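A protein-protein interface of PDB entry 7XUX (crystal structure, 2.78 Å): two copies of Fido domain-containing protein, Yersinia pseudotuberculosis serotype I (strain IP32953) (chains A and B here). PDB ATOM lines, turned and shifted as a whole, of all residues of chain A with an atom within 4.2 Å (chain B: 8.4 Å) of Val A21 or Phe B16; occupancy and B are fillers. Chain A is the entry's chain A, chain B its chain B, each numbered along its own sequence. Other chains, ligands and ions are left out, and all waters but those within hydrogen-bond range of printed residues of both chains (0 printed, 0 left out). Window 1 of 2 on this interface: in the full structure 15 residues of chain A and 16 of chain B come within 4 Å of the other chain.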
ATOM      1  N   ASN A  13      17.175   8.193  -7.843  1.00  0.00           N
ATOM      2  CA  ASN A  13      16.203   7.098  -7.856  1.00  0.00           C
ATOM      3  C   ASN A  13      15.583   6.963  -6.473  1.00  0.00           C
ATOM      4  O   ASN A  13      15.881   6.027  -5.722  1.00  0.00           O
ATOM      5  CB  ASN A  13      16.865   5.792  -8.292  1.00  0.00           C
ATOM      6  CG  ASN A  13      15.865   4.674  -8.507  1.00  0.00           C
ATOM      7  OD1 ASN A  13      14.763   4.899  -9.008  1.00  0.00           O
ATOM      8  ND2 ASN A  13      16.244   3.460  -8.128  1.00  0.00           N
ATOM      9  N   PRO A  14      14.700   7.888  -6.101  1.00  0.00           N
ATOM     10  CA  PRO A  14      14.031   7.790  -4.804  1.00  0.00           C
ATOM     11  C   PRO A  14      12.876   6.800  -4.844  1.00  0.00           C
ATOM     12  O   PRO A  14      12.401   6.390  -5.904  1.00  0.00           O
ATOM     13  CB  PRO A  14      13.526   9.215  -4.561  1.00  0.00           C
ATOM     14  CG  PRO A  14      13.287   9.755  -5.929  1.00  0.00           C
ATOM     15  CD  PRO A  14      14.258   9.069  -6.864  1.00  0.00           C
ATOM     16  N   SER A  15      12.428   6.419  -3.651  1.00  0.00           N
ATOM     17  CA  SER A  15      11.330   5.476  -3.533  1.00  0.00           C
ATOM     18  C   SER A  15       9.987   6.200  -3.627  1.00  0.00           C
ATOM     19  O   SER A  15       9.902   7.429  -3.565  1.00  0.00           O
ATOM     20  CB  SER A  15      11.433   4.693  -2.225  1.00  0.00           C
ATOM     21  OG  SER A  15      12.720   4.837  -1.650  1.00  0.00           O
ATOM     22  N   PHE A  16       8.924   5.406  -3.779  1.00  0.00           N
ATOM     23  CA  PHE A  16       7.594   5.967  -3.995  1.00  0.00           C
ATOM     24  C   PHE A  16       7.116   6.785  -2.802  1.00  0.00           C
ATOM     25  O   PHE A  16       6.355   7.744  -2.977  1.00  0.00           O
ATOM     26  CB  PHE A  16       6.605   4.842  -4.305  1.00  0.00           C
ATOM     27  CG  PHE A  16       5.259   5.322  -4.771  1.00  0.00           C
ATOM     28  CD1 PHE A  16       5.064   5.715  -6.085  1.00  0.00           C
ATOM     29  CD2 PHE A  16       4.185   5.365  -3.899  1.00  0.00           C
ATOM     30  CE1 PHE A  16       3.825   6.151  -6.516  1.00  0.00           C
ATOM     31  CE2 PHE A  16       2.945   5.799  -4.324  1.00  0.00           C
ATOM     32  CZ  PHE A  16       2.764   6.193  -5.634  1.00  0.00           C
ATOM     33  N   SER A  18       8.729   8.849  -1.087  1.00  0.00           N
ATOM     34  CA  SER A  18       9.548  10.025  -0.852  1.00  0.00           C
ATOM     35  C   SER A  18       8.784  11.300  -1.197  1.00  0.00           C
ATOM     36  O   SER A  18       7.927  11.300  -2.086  1.00  0.00           O
ATOM     37  CB  SER A  18      10.824   9.957  -1.684  1.00  0.00           C
ATOM     38  OG  SER A  18      10.523   9.859  -3.065  1.00  0.00           O
ATOM     39  N   PRO A  19       9.075  12.401  -0.500  1.00  0.00           N
ATOM     40  CA  PRO A  19       8.496  13.694  -0.900  1.00  0.00           C
ATOM     41  C   PRO A  19       8.952  14.154  -2.272  1.00  0.00           C
ATOM     42  O   PRO A  19       8.253  14.954  -2.907  1.00  0.00           O
ATOM     43  CB  PRO A  19       8.976  14.651   0.200  1.00  0.00           C
ATOM     44  CG  PRO A  19       9.326  13.767   1.357  1.00  0.00           C
ATOM     45  CD  PRO A  19       9.849  12.504   0.747  1.00  0.00           C
ATOM     46  N   LEU A  20      10.105  13.676  -2.749  1.00  0.00           N
ATOM     47  CA  LEU A  20      10.572  14.055  -4.079  1.00  0.00           C
ATOM     48  C   LEU A  20       9.680  13.466  -5.164  1.00  0.00           C
ATOM     49  O   LEU A  20       9.405  14.126  -6.173  1.00  0.00           O
ATOM     50  CB  LEU A  20      12.021  13.611  -4.273  1.00  0.00           C
ATOM     51  CG  LEU A  20      12.673  13.998  -5.601  1.00  0.00           C
ATOM     52  CD1 LEU A  20      12.812  15.508  -5.705  1.00  0.00           C
ATOM     53  CD2 LEU A  20      14.025  13.321  -5.754  1.00  0.00           C
ATOM     54  N   VAL A  21       9.224  12.225  -4.977  1.00  0.00           N
ATOM     55  CA  VAL A  21       8.287  11.626  -5.923  1.00  0.00           C
ATOM     56  C   VAL A  21       6.979  12.404  -5.938  1.00  0.00           C
ATOM     57  O   VAL A  21       6.350  12.562  -6.992  1.00  0.00           O
ATOM     58  CB  VAL A  21       8.074  10.136  -5.584  1.00  0.00           C
ATOM     59  CG1 VAL A  21       6.695   9.659  -6.027  1.00  0.00           C
ATOM     60  CG2 VAL A  21       9.166   9.288  -6.221  1.00  0.00           C
ATOM     61  N   ASP A  22       6.561  12.924  -4.780  1.00  0.00           N
ATOM     62  CA  ASP A  22       5.358  13.748  -4.724  1.00  0.00           C
ATOM     63  C   ASP A  22       5.507  14.994  -5.587  1.00  0.00           C
ATOM     64  O   ASP A  22       4.631  15.310  -6.399  1.00  0.00           O
ATOM     65  CB  ASP A  22       5.052  14.128  -3.275  1.00  0.00           C
ATOM     66  CG  ASP A  22       4.688  12.931  -2.423  1.00  0.00           C
ATOM     67  OD1 ASP A  22       4.175  11.940  -2.985  1.00  0.00           O
ATOM     68  OD2 ASP A  22       4.916  12.977  -1.196  1.00  0.00           O
ATOM     69  N   ALA A  23       6.620  15.714  -5.427  1.00  0.00           N
ATOM     70  CA  ALA A  23       6.855  16.902  -6.241  1.00  0.00           C
ATOM     71  C   ALA A  23       7.058  16.550  -7.708  1.00  0.00           C
ATOM     72  O   ALA A  23       6.686  17.333  -8.589  1.00  0.00           O
ATOM     73  CB  ALA A  23       8.062  17.674  -5.713  1.00  0.00           C
ATOM     74  N   LEU A  24       7.643  15.384  -7.989  1.00  0.00           N
ATOM     75  CA  LEU A  24       7.870  14.977  -9.373  1.00  0.00           C
ATOM     76  C   LEU A  24       6.551  14.729 -10.095  1.00  0.00           C
ATOM     77  O   LEU A  24       6.346  15.207 -11.218  1.00  0.00           O
ATOM     78  CB  LEU A  24       8.752  13.729  -9.409  1.00  0.00           C
ATOM     79  CG  LEU A  24      10.245  13.961  -9.650  1.00  0.00           C
ATOM     80  CD1 LEU A  24      11.062  12.770  -9.183  1.00  0.00           C
ATOM     81  CD2 LEU A  24      10.513  14.257 -11.120  1.00  0.00           C
ATOM     82  N   THR A  25       5.641  13.984  -9.463  1.00  0.00           N
ATOM     83  CA  THR A  25       4.335  13.745 -10.069  1.00  0.00           C
ATOM     84  C   THR A  25       3.490  15.012 -10.069  1.00  0.00           C
ATOM     85  O   THR A  25       2.725  15.253 -11.010  1.00  0.00           O
ATOM     86  CB  THR A  25       3.609  12.621  -9.330  1.00  0.00           C
ATOM     87  OG1 THR A  25       3.323  13.039  -7.989  1.00  0.00           O
ATOM     88  CG2 THR A  25       4.472  11.374  -9.285  1.00  0.00           C
ATOM     89  N   LYS A 175      10.000  10.956 -17.633  1.00  0.00           N
ATOM     90  CA  LYS A 175       9.822  11.199 -16.206  1.00  0.00           C
ATOM     91  C   LYS A 175      11.053  11.838 -15.578  1.00  0.00           C
ATOM     92  O   LYS A 175      10.932  12.514 -14.552  1.00  0.00           O
ATOM     93  CB  LYS A 175       9.490   9.892 -15.483  1.00  0.00           C
ATOM     94  CG  LYS A 175      10.519   8.789 -15.685  1.00  0.00           C
ATOM     95  CD  LYS A 175      10.364   7.687 -14.650  1.00  0.00           C
ATOM     96  CE  LYS A 175      11.083   6.419 -15.084  1.00  0.00           C
ATOM     97  NZ  LYS A 175      10.683   5.239 -14.268  1.00  0.00           N
ATOM     98  N   TYR A 176      12.230  11.644 -16.180  1.00  0.00           N
ATOM     99  CA  TYR A 176      13.479  12.198 -15.674  1.00  0.00           C
ATOM    100  C   TYR A 176      13.719  13.636 -16.116  1.00  0.00           C
ATOM    101  O   TYR A 176      14.694  14.246 -15.664  1.00  0.00           O
ATOM    102  CB  TYR A 176      14.660  11.336 -16.134  1.00  0.00           C
ATOM    103  CG  TYR A 176      14.663   9.920 -15.598  1.00  0.00           C
ATOM    104  CD1 TYR A 176      14.699   9.673 -14.235  1.00  0.00           C
ATOM    105  CD2 TYR A 176      14.648   8.830 -16.459  1.00  0.00           C
ATOM    106  CE1 TYR A 176      14.708   8.384 -13.738  1.00  0.00           C
ATOM    107  CE2 TYR A 176      14.656   7.533 -15.972  1.00  0.00           C
ATOM    108  CZ  TYR A 176      14.687   7.318 -14.610  1.00  0.00           C
ATOM    109  OH  TYR A 176      14.696   6.034 -14.114  1.00  0.00           O
ATOM    110  N   ASN B  13       6.008  -0.270  -2.399  1.00  0.00           N
ATOM    111  CA  ASN B  13       6.939   0.854  -2.476  1.00  0.00           C
ATOM    112  C   ASN B  13       7.962   0.588  -3.565  1.00  0.00           C
ATOM    113  O   ASN B  13       9.057   0.072  -3.302  1.00  0.00           O
ATOM    114  CB  ASN B  13       7.632   1.107  -1.141  1.00  0.00           C
ATOM    115  CG  ASN B  13       8.639   2.223  -1.232  1.00  0.00           C
ATOM    116  OD1 ASN B  13       8.481   3.144  -2.033  1.00  0.00           O
ATOM    117  ND2 ASN B  13       9.675   2.160  -0.405  1.00  0.00           N
ATOM    118  N   PRO B  14       7.647   0.942  -4.804  1.00  0.00           N
ATOM    119  CA  PRO B  14       8.616   0.781  -5.888  1.00  0.00           C
ATOM    120  C   PRO B  14       9.557   1.973  -5.982  1.00  0.00           C
ATOM    121  O   PRO B  14       9.287   3.064  -5.473  1.00  0.00           O
ATOM    122  CB  PRO B  14       7.740   0.675  -7.144  1.00  0.00           C
ATOM    123  CG  PRO B  14       6.328   1.021  -6.708  1.00  0.00           C
ATOM    124  CD  PRO B  14       6.360   1.467  -5.284  1.00  0.00           C
ATOM    125  N   SER B  15      10.684   1.740  -6.646  1.00  0.00           N
ATOM    126  CA  SER B  15      11.637   2.804  -6.908  1.00  0.00           C
ATOM    127  C   SER B  15      11.181   3.637  -8.102  1.00  0.00           C
ATOM    128  O   SER B  15      10.357   3.208  -8.914  1.00  0.00           O
ATOM    129  CB  SER B  15      13.030   2.229  -7.168  1.00  0.00           C
ATOM    130  OG  SER B  15      13.569   1.646  -5.993  1.00  0.00           O
ATOM    131  N   PHE B  16      11.734   4.850  -8.201  1.00  0.00           N
ATOM    132  CA  PHE B  16      11.330   5.761  -9.267  1.00  0.00           C
ATOM    133  C   PHE B  16      11.640   5.195 -10.648  1.00  0.00           C
ATOM    134  O   PHE B  16      10.968   5.544 -11.624  1.00  0.00           O
ATOM    135  CB  PHE B  16      12.012   7.117  -9.083  1.00  0.00           C
ATOM    136  CG  PHE B  16      11.489   8.189  -9.996  1.00  0.00           C
ATOM    137  CD1 PHE B  16      10.275   8.807  -9.737  1.00  0.00           C
ATOM    138  CD2 PHE B  16      12.209   8.579 -11.112  1.00  0.00           C
ATOM    139  CE1 PHE B  16       9.791   9.792 -10.577  1.00  0.00           C
ATOM    140  CE2 PHE B  16      11.730   9.566 -11.955  1.00  0.00           C
ATOM    141  CZ  PHE B  16      10.519  10.172 -11.687  1.00  0.00           C
ATOM    142  N   ASP B  17      12.642   4.321 -10.750  1.00  0.00           N
ATOM    143  CA  ASP B  17      13.024   3.750 -12.036  1.00  0.00           C
ATOM    144  C   ASP B  17      12.074   2.663 -12.522  1.00  0.00           C
ATOM    145  O   ASP B  17      12.232   2.188 -13.651  1.00  0.00           O
ATOM    146  CB  ASP B  17      14.455   3.195 -11.962  1.00  0.00           C
ATOM    147  CG  ASP B  17      14.584   1.979 -11.041  1.00  0.00           C
ATOM    148  OD1 ASP B  17      13.568   1.491 -10.498  1.00  0.00           O
ATOM    149  OD2 ASP B  17      15.723   1.499 -10.865  1.00  0.00           O
ATOM    150  N   SER B  18      11.101   2.260 -11.704  1.00  0.00           N
ATOM    151  CA  SER B  18      10.273   1.094 -11.975  1.00  0.00           C
ATOM    152  C   SER B  18       9.107   1.442 -12.894  1.00  0.00           C
ATOM    153  O   SER B  18       8.581   2.559 -12.851  1.00  0.00           O
ATOM    154  CB  SER B  18       9.734   0.514 -10.671  1.00  0.00           C
ATOM    155  OG  SER B  18       8.701   1.328 -10.145  1.00  0.00           O
ATOM    156  N   PRO B  19       8.692   0.490 -13.736  1.00  0.00           N
ATOM    157  CA  PRO B  19       7.500   0.718 -14.570  1.00  0.00           C
ATOM    158  C   PRO B  19       6.218   0.854 -13.768  1.00  0.00           C
ATOM    159  O   PRO B  19       5.247   1.422 -14.282  1.00  0.00           O
ATOM    160  CB  PRO B  19       7.448  -0.515 -15.484  1.00  0.00           C
ATOM    161  CG  PRO B  19       8.439  -1.484 -14.954  1.00  0.00           C
ATOM    162  CD  PRO B  19       9.357  -0.795 -14.006  1.00  0.00           C
ATOM    163  N   LEU B  20       6.177   0.344 -12.534  1.00  0.00           N
ATOM    164  CA  LEU B  20       4.993   0.519 -11.700  1.00  0.00           C
ATOM    165  C   LEU B  20       4.762   1.991 -11.386  1.00  0.00           C
ATOM    166  O   LEU B  20       3.620   2.465 -11.401  1.00  0.00           O
ATOM    167  CB  LEU B  20       5.134  -0.297 -10.413  1.00  0.00           C
ATOM    168  CG  LEU B  20       4.029  -0.221  -9.355  1.00  0.00           C
ATOM    169  CD1 LEU B  20       2.646  -0.274  -9.984  1.00  0.00           C
ATOM    170  CD2 LEU B  20       4.196  -1.348  -8.346  1.00  0.00           C
ATOM    171  N   VAL B  21       5.835   2.730 -11.101  1.00  0.00           N
ATOM    172  CA  VAL B  21       5.706   4.166 -10.878  1.00  0.00           C
ATOM    173  C   VAL B  21       5.264   4.864 -12.159  1.00  0.00           C
ATOM    174  O   VAL B  21       4.492   5.829 -12.121  1.00  0.00           O
ATOM    175  CB  VAL B  21       7.028   4.740 -10.335  1.00  0.00           C
ATOM    176  CG1 VAL B  21       6.985   6.260 -10.295  1.00  0.00           C
ATOM    177  CG2 VAL B  21       7.310   4.180  -8.951  1.00  0.00           C
ATOM    178  N   ASP B  22       5.729   4.377 -13.313  1.00  0.00           N
ATOM    179  CA  ASP B  22       5.307   4.950 -14.588  1.00  0.00           C
ATOM    180  C   ASP B  22       3.797   4.846 -14.763  1.00  0.00           C
ATOM    181  O   ASP B  22       3.132   5.821 -15.131  1.00  0.00           O
ATOM    182  CB  ASP B  22       6.028   4.252 -15.742  1.00  0.00           C
ATOM    183  CG  ASP B  22       7.521   4.508 -15.738  1.00  0.00           C
ATOM    184  OD1 ASP B  22       8.012   5.160 -14.794  1.00  0.00           O
ATOM    185  OD2 ASP B  22       8.204   4.056 -16.682  1.00  0.00           O
ATOM    186  N   LEU B  24       1.593   4.443 -12.405  1.00  0.00           N
ATOM    187  CA  LEU B  24       0.884   5.140 -11.336  1.00  0.00           C
ATOM    188  C   LEU B  24       0.684   6.612 -11.675  1.00  0.00           C
ATOM    189  O   LEU B  24      -0.410   7.159 -11.493  1.00  0.00           O
ATOM    190  CB  LEU B  24       1.643   4.987 -10.016  1.00  0.00           C
ATOM    191  CG  LEU B  24       1.367   3.713  -9.213  1.00  0.00           C
ATOM    192  CD1 LEU B  24       2.592   3.308  -8.408  1.00  0.00           C
ATOM    193  CD2 LEU B  24       0.168   3.908  -8.300  1.00  0.00           C
ATOM    194  N   THR B  25       1.736   7.277 -12.165  1.00  0.00           N
ATOM    195  CA  THR B  25       1.604   8.677 -12.556  1.00  0.00           C
ATOM    196  C   THR B  25       0.698   8.824 -13.771  1.00  0.00           C
ATOM    197  O   THR B  25      -0.105   9.763 -13.843  1.00  0.00           O
ATOM    198  CB  THR B  25       2.977   9.282 -12.849  1.00  0.00           C
ATOM    199  OG1 THR B  25       3.443   8.813 -14.120  1.00  0.00           O
ATOM    200  CG2 THR B  25       3.972   8.887 -11.775  1.00  0.00           C
ATOM    201  N   LYS B 175      -1.886   9.375  -3.487  1.00  0.00           N
ATOM    202  CA  LYS B 175      -1.044   8.699  -4.470  1.00  0.00           C
ATOM    203  C   LYS B 175      -1.185   7.185  -4.370  1.00  0.00           C
ATOM    204  O   LYS B 175      -0.981   6.476  -5.362  1.00  0.00           O
ATOM    205  CB  LYS B 175       0.418   9.110  -4.288  1.00  0.00           C
ATOM    206  CG  LYS B 175       0.875   9.150  -2.839  1.00  0.00           C
ATOM    207  CD  LYS B 175       2.356   8.826  -2.713  1.00  0.00           C
ATOM    208  CE  LYS B 175       2.950   9.419  -1.447  1.00  0.00           C
ATOM    209  NZ  LYS B 175       4.397   9.096  -1.311  1.00  0.00           N
ATOM    210  N   TYR B 176      -1.545   6.680  -3.191  1.00  0.00           N
ATOM    211  CA  TYR B 176      -1.725   5.254  -2.951  1.00  0.00           C
ATOM    212  C   TYR B 176      -3.118   4.758  -3.314  1.00  0.00           C
ATOM    213  O   TYR B 176      -3.396   3.566  -3.146  1.00  0.00           O
ATOM    214  CB  TYR B 176      -1.450   4.934  -1.479  1.00  0.00           C
ATOM    215  CG  TYR B 176       0.007   4.983  -1.083  1.00  0.00           C
ATOM    216  CD1 TYR B 176       0.934   4.126  -1.660  1.00  0.00           C
ATOM    217  CD2 TYR B 176       0.455   5.884  -0.126  1.00  0.00           C
ATOM    218  CE1 TYR B 176       2.267   4.167  -1.297  1.00  0.00           C
ATOM    219  CE2 TYR B 176       1.785   5.933   0.244  1.00  0.00           C
ATOM    220  CZ  TYR B 176       2.686   5.072  -0.345  1.00  0.00           C
ATOM    221  OH  TYR B 176       4.013   5.117   0.019  1.00  0.00           O
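The backbone NH (N) of Phe B16 lies within hydrogen-bond range of the side-chain amide oxygen (OD1) of Asn A13 (3.1 Å).
The side-chain amide oxygen (OD1) of Asn A13 sits at hydrogen-bond distance from the backbone NH (N) of Asp B17.
The backbone NH (N) of Phe B16 lies within hydrogen-bond range of the backbone carbonyl oxygen (O) of Pro A14 (2.8 Å).
The side-chain amide oxygen of Asn B13 sits at hydrogen-bond distance from the backbone NH of Phe A16 (2.9 Å).
The backbone NH of Phe A16 lies within hydrogen-bond range of the backbone carbonyl oxygen of Pro B14, at 2.9 Å.
NZ of Lys B175 is in hydrogen-bond range of O of Phe A16 (2.9 Å).
The side-chain amino group (NZ) of Lys B175 lies within salt-bridge range of the side-chain carboxylate (OD1) of Asp A22.
The side-chain amino group (NZ) of Lys A175 is in hydrogen-bond range of the backbone carbonyl oxygen (O) of Phe B16, at 2.7 Å.
The side-chain amino group of Lys A175 sits close to the backbone carbonyl oxygen of Asp B17 (3.5 Å).
OD1 of Asp B22 is in salt-bridge range of NZ of Lys A175 (2.7 Å).
The backbone NH of Val A21 sits at hydrogen-bond distance from the side-chain hydroxyl of Ser A18.
The backbone carbonyl oxygen (O) of Val A21 lies close to the side-chain hydroxyl (OG1) of Thr A25 (3.2 Å).
The backbone carbonyl oxygen of Asp A22 is in hydrogen-bond range of the side-chain hydroxyl of Thr A25 (3.1 Å).
The side-chain hydroxyl (OG) of Ser B18 is in hydrogen-bond range of the backbone carbonyl oxygen (O) of Ser B15.
The backbone NH of Val B21 sits at hydrogen-bond distance from the side-chain hydroxyl of Ser B18, 3.3 Å away.
OG1 of Thr B25 lies within hydrogen-bond range of O of Asp B22 (3.2 Å).
Among the printed residues, merely in contact across the chains: Asn A13 with Ser B15 (3.6 Å), Pro A14 with Ser B15 (3.7 Å), Ser A15 with Asn B13 (3.3 Å), Ser A15 with Pro B14 (3.7 Å), Phe A16 with Val B21 (3.95 Å), Phe A16 with Leu B24 (3.6 Å), Phe A16 with Tyr B176 (3.4 Å), Val A21 with Phe B16 (3.7 Å), Leu A24 with Phe B16 (3.5 Å), Thr A25 with Thr B25 (3.6 Å), Lys A175 with Ser B18 (3.7 Å), Tyr A176 with Phe B16 (3.6 Å) and Tyr A176 with Asp B17 (3.5 Å).
Val A21 touches just one residue of chain B: Phe B16 (3.7 Å).
Of the printed residues of chain B, Thr A25 touches Thr B25.
Printed residues of chain A within 4 Å of Asn B13: Ser A15 and Phe A16.
Of chain A, only Asn A13 (3.1 Å), Pro A14 (2.8 Å), Val A21 (3.7 Å), Leu A24 (3.5 Å), Lys A175 (2.7 Å) and Tyr A176 (3.6 Å) come within 4 Å of Phe B16.
Of the printed residues of chain A, Asp B17 touches Asn A13 (2.8 Å), Lys A175 (3.4 Å) and Tyr A176 (3.5 Å).
The nearest residue of chain B that does not touch Val A21 is Lys B175 (5.3 Å).
The nearest printed residue of chain A that does not touch Phe B16 is Ser A15 (4.7 Å).
Printed residues of chain B that touch a printed residue of chain A: Asn B13, Pro B14, Ser B15, Phe B16, Asp B17, Ser B18, Val B21, Asp B22, Leu B24, Thr B25, Lys B175 and Tyr B176.
Among the printed residues, Asp or Glu carboxylates within 4 Å of a Lys or Arg side-chain nitrogen of the other chain: Asp A22 with Lys B175 (3.3 Å) and Lys A175 with Asp B22 (2.7 Å).
Phe A16 touches Leu B24, and with the chains exchanged Leu A24 touches Phe B16.
Phe A16 touches Lys B175, and with the chains exchanged Lys A175 touches Phe B16.
Phe A16 touches Tyr B176, and with the chains exchanged Tyr A176 touches Phe B16.
Lys A175 touches Ser B18, but with the chains exchanged Ser A18 does not touch Lys B175 (4.2 Å).
Positions printed for both chains: 13, 14, 15, 16, 18, 19, 20, 21, 22, 24, 25, 175 and 176.
Of the 23 pairs that touch across the chains among the printed residues, 19 have their exchanged pair printed and touching as well.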
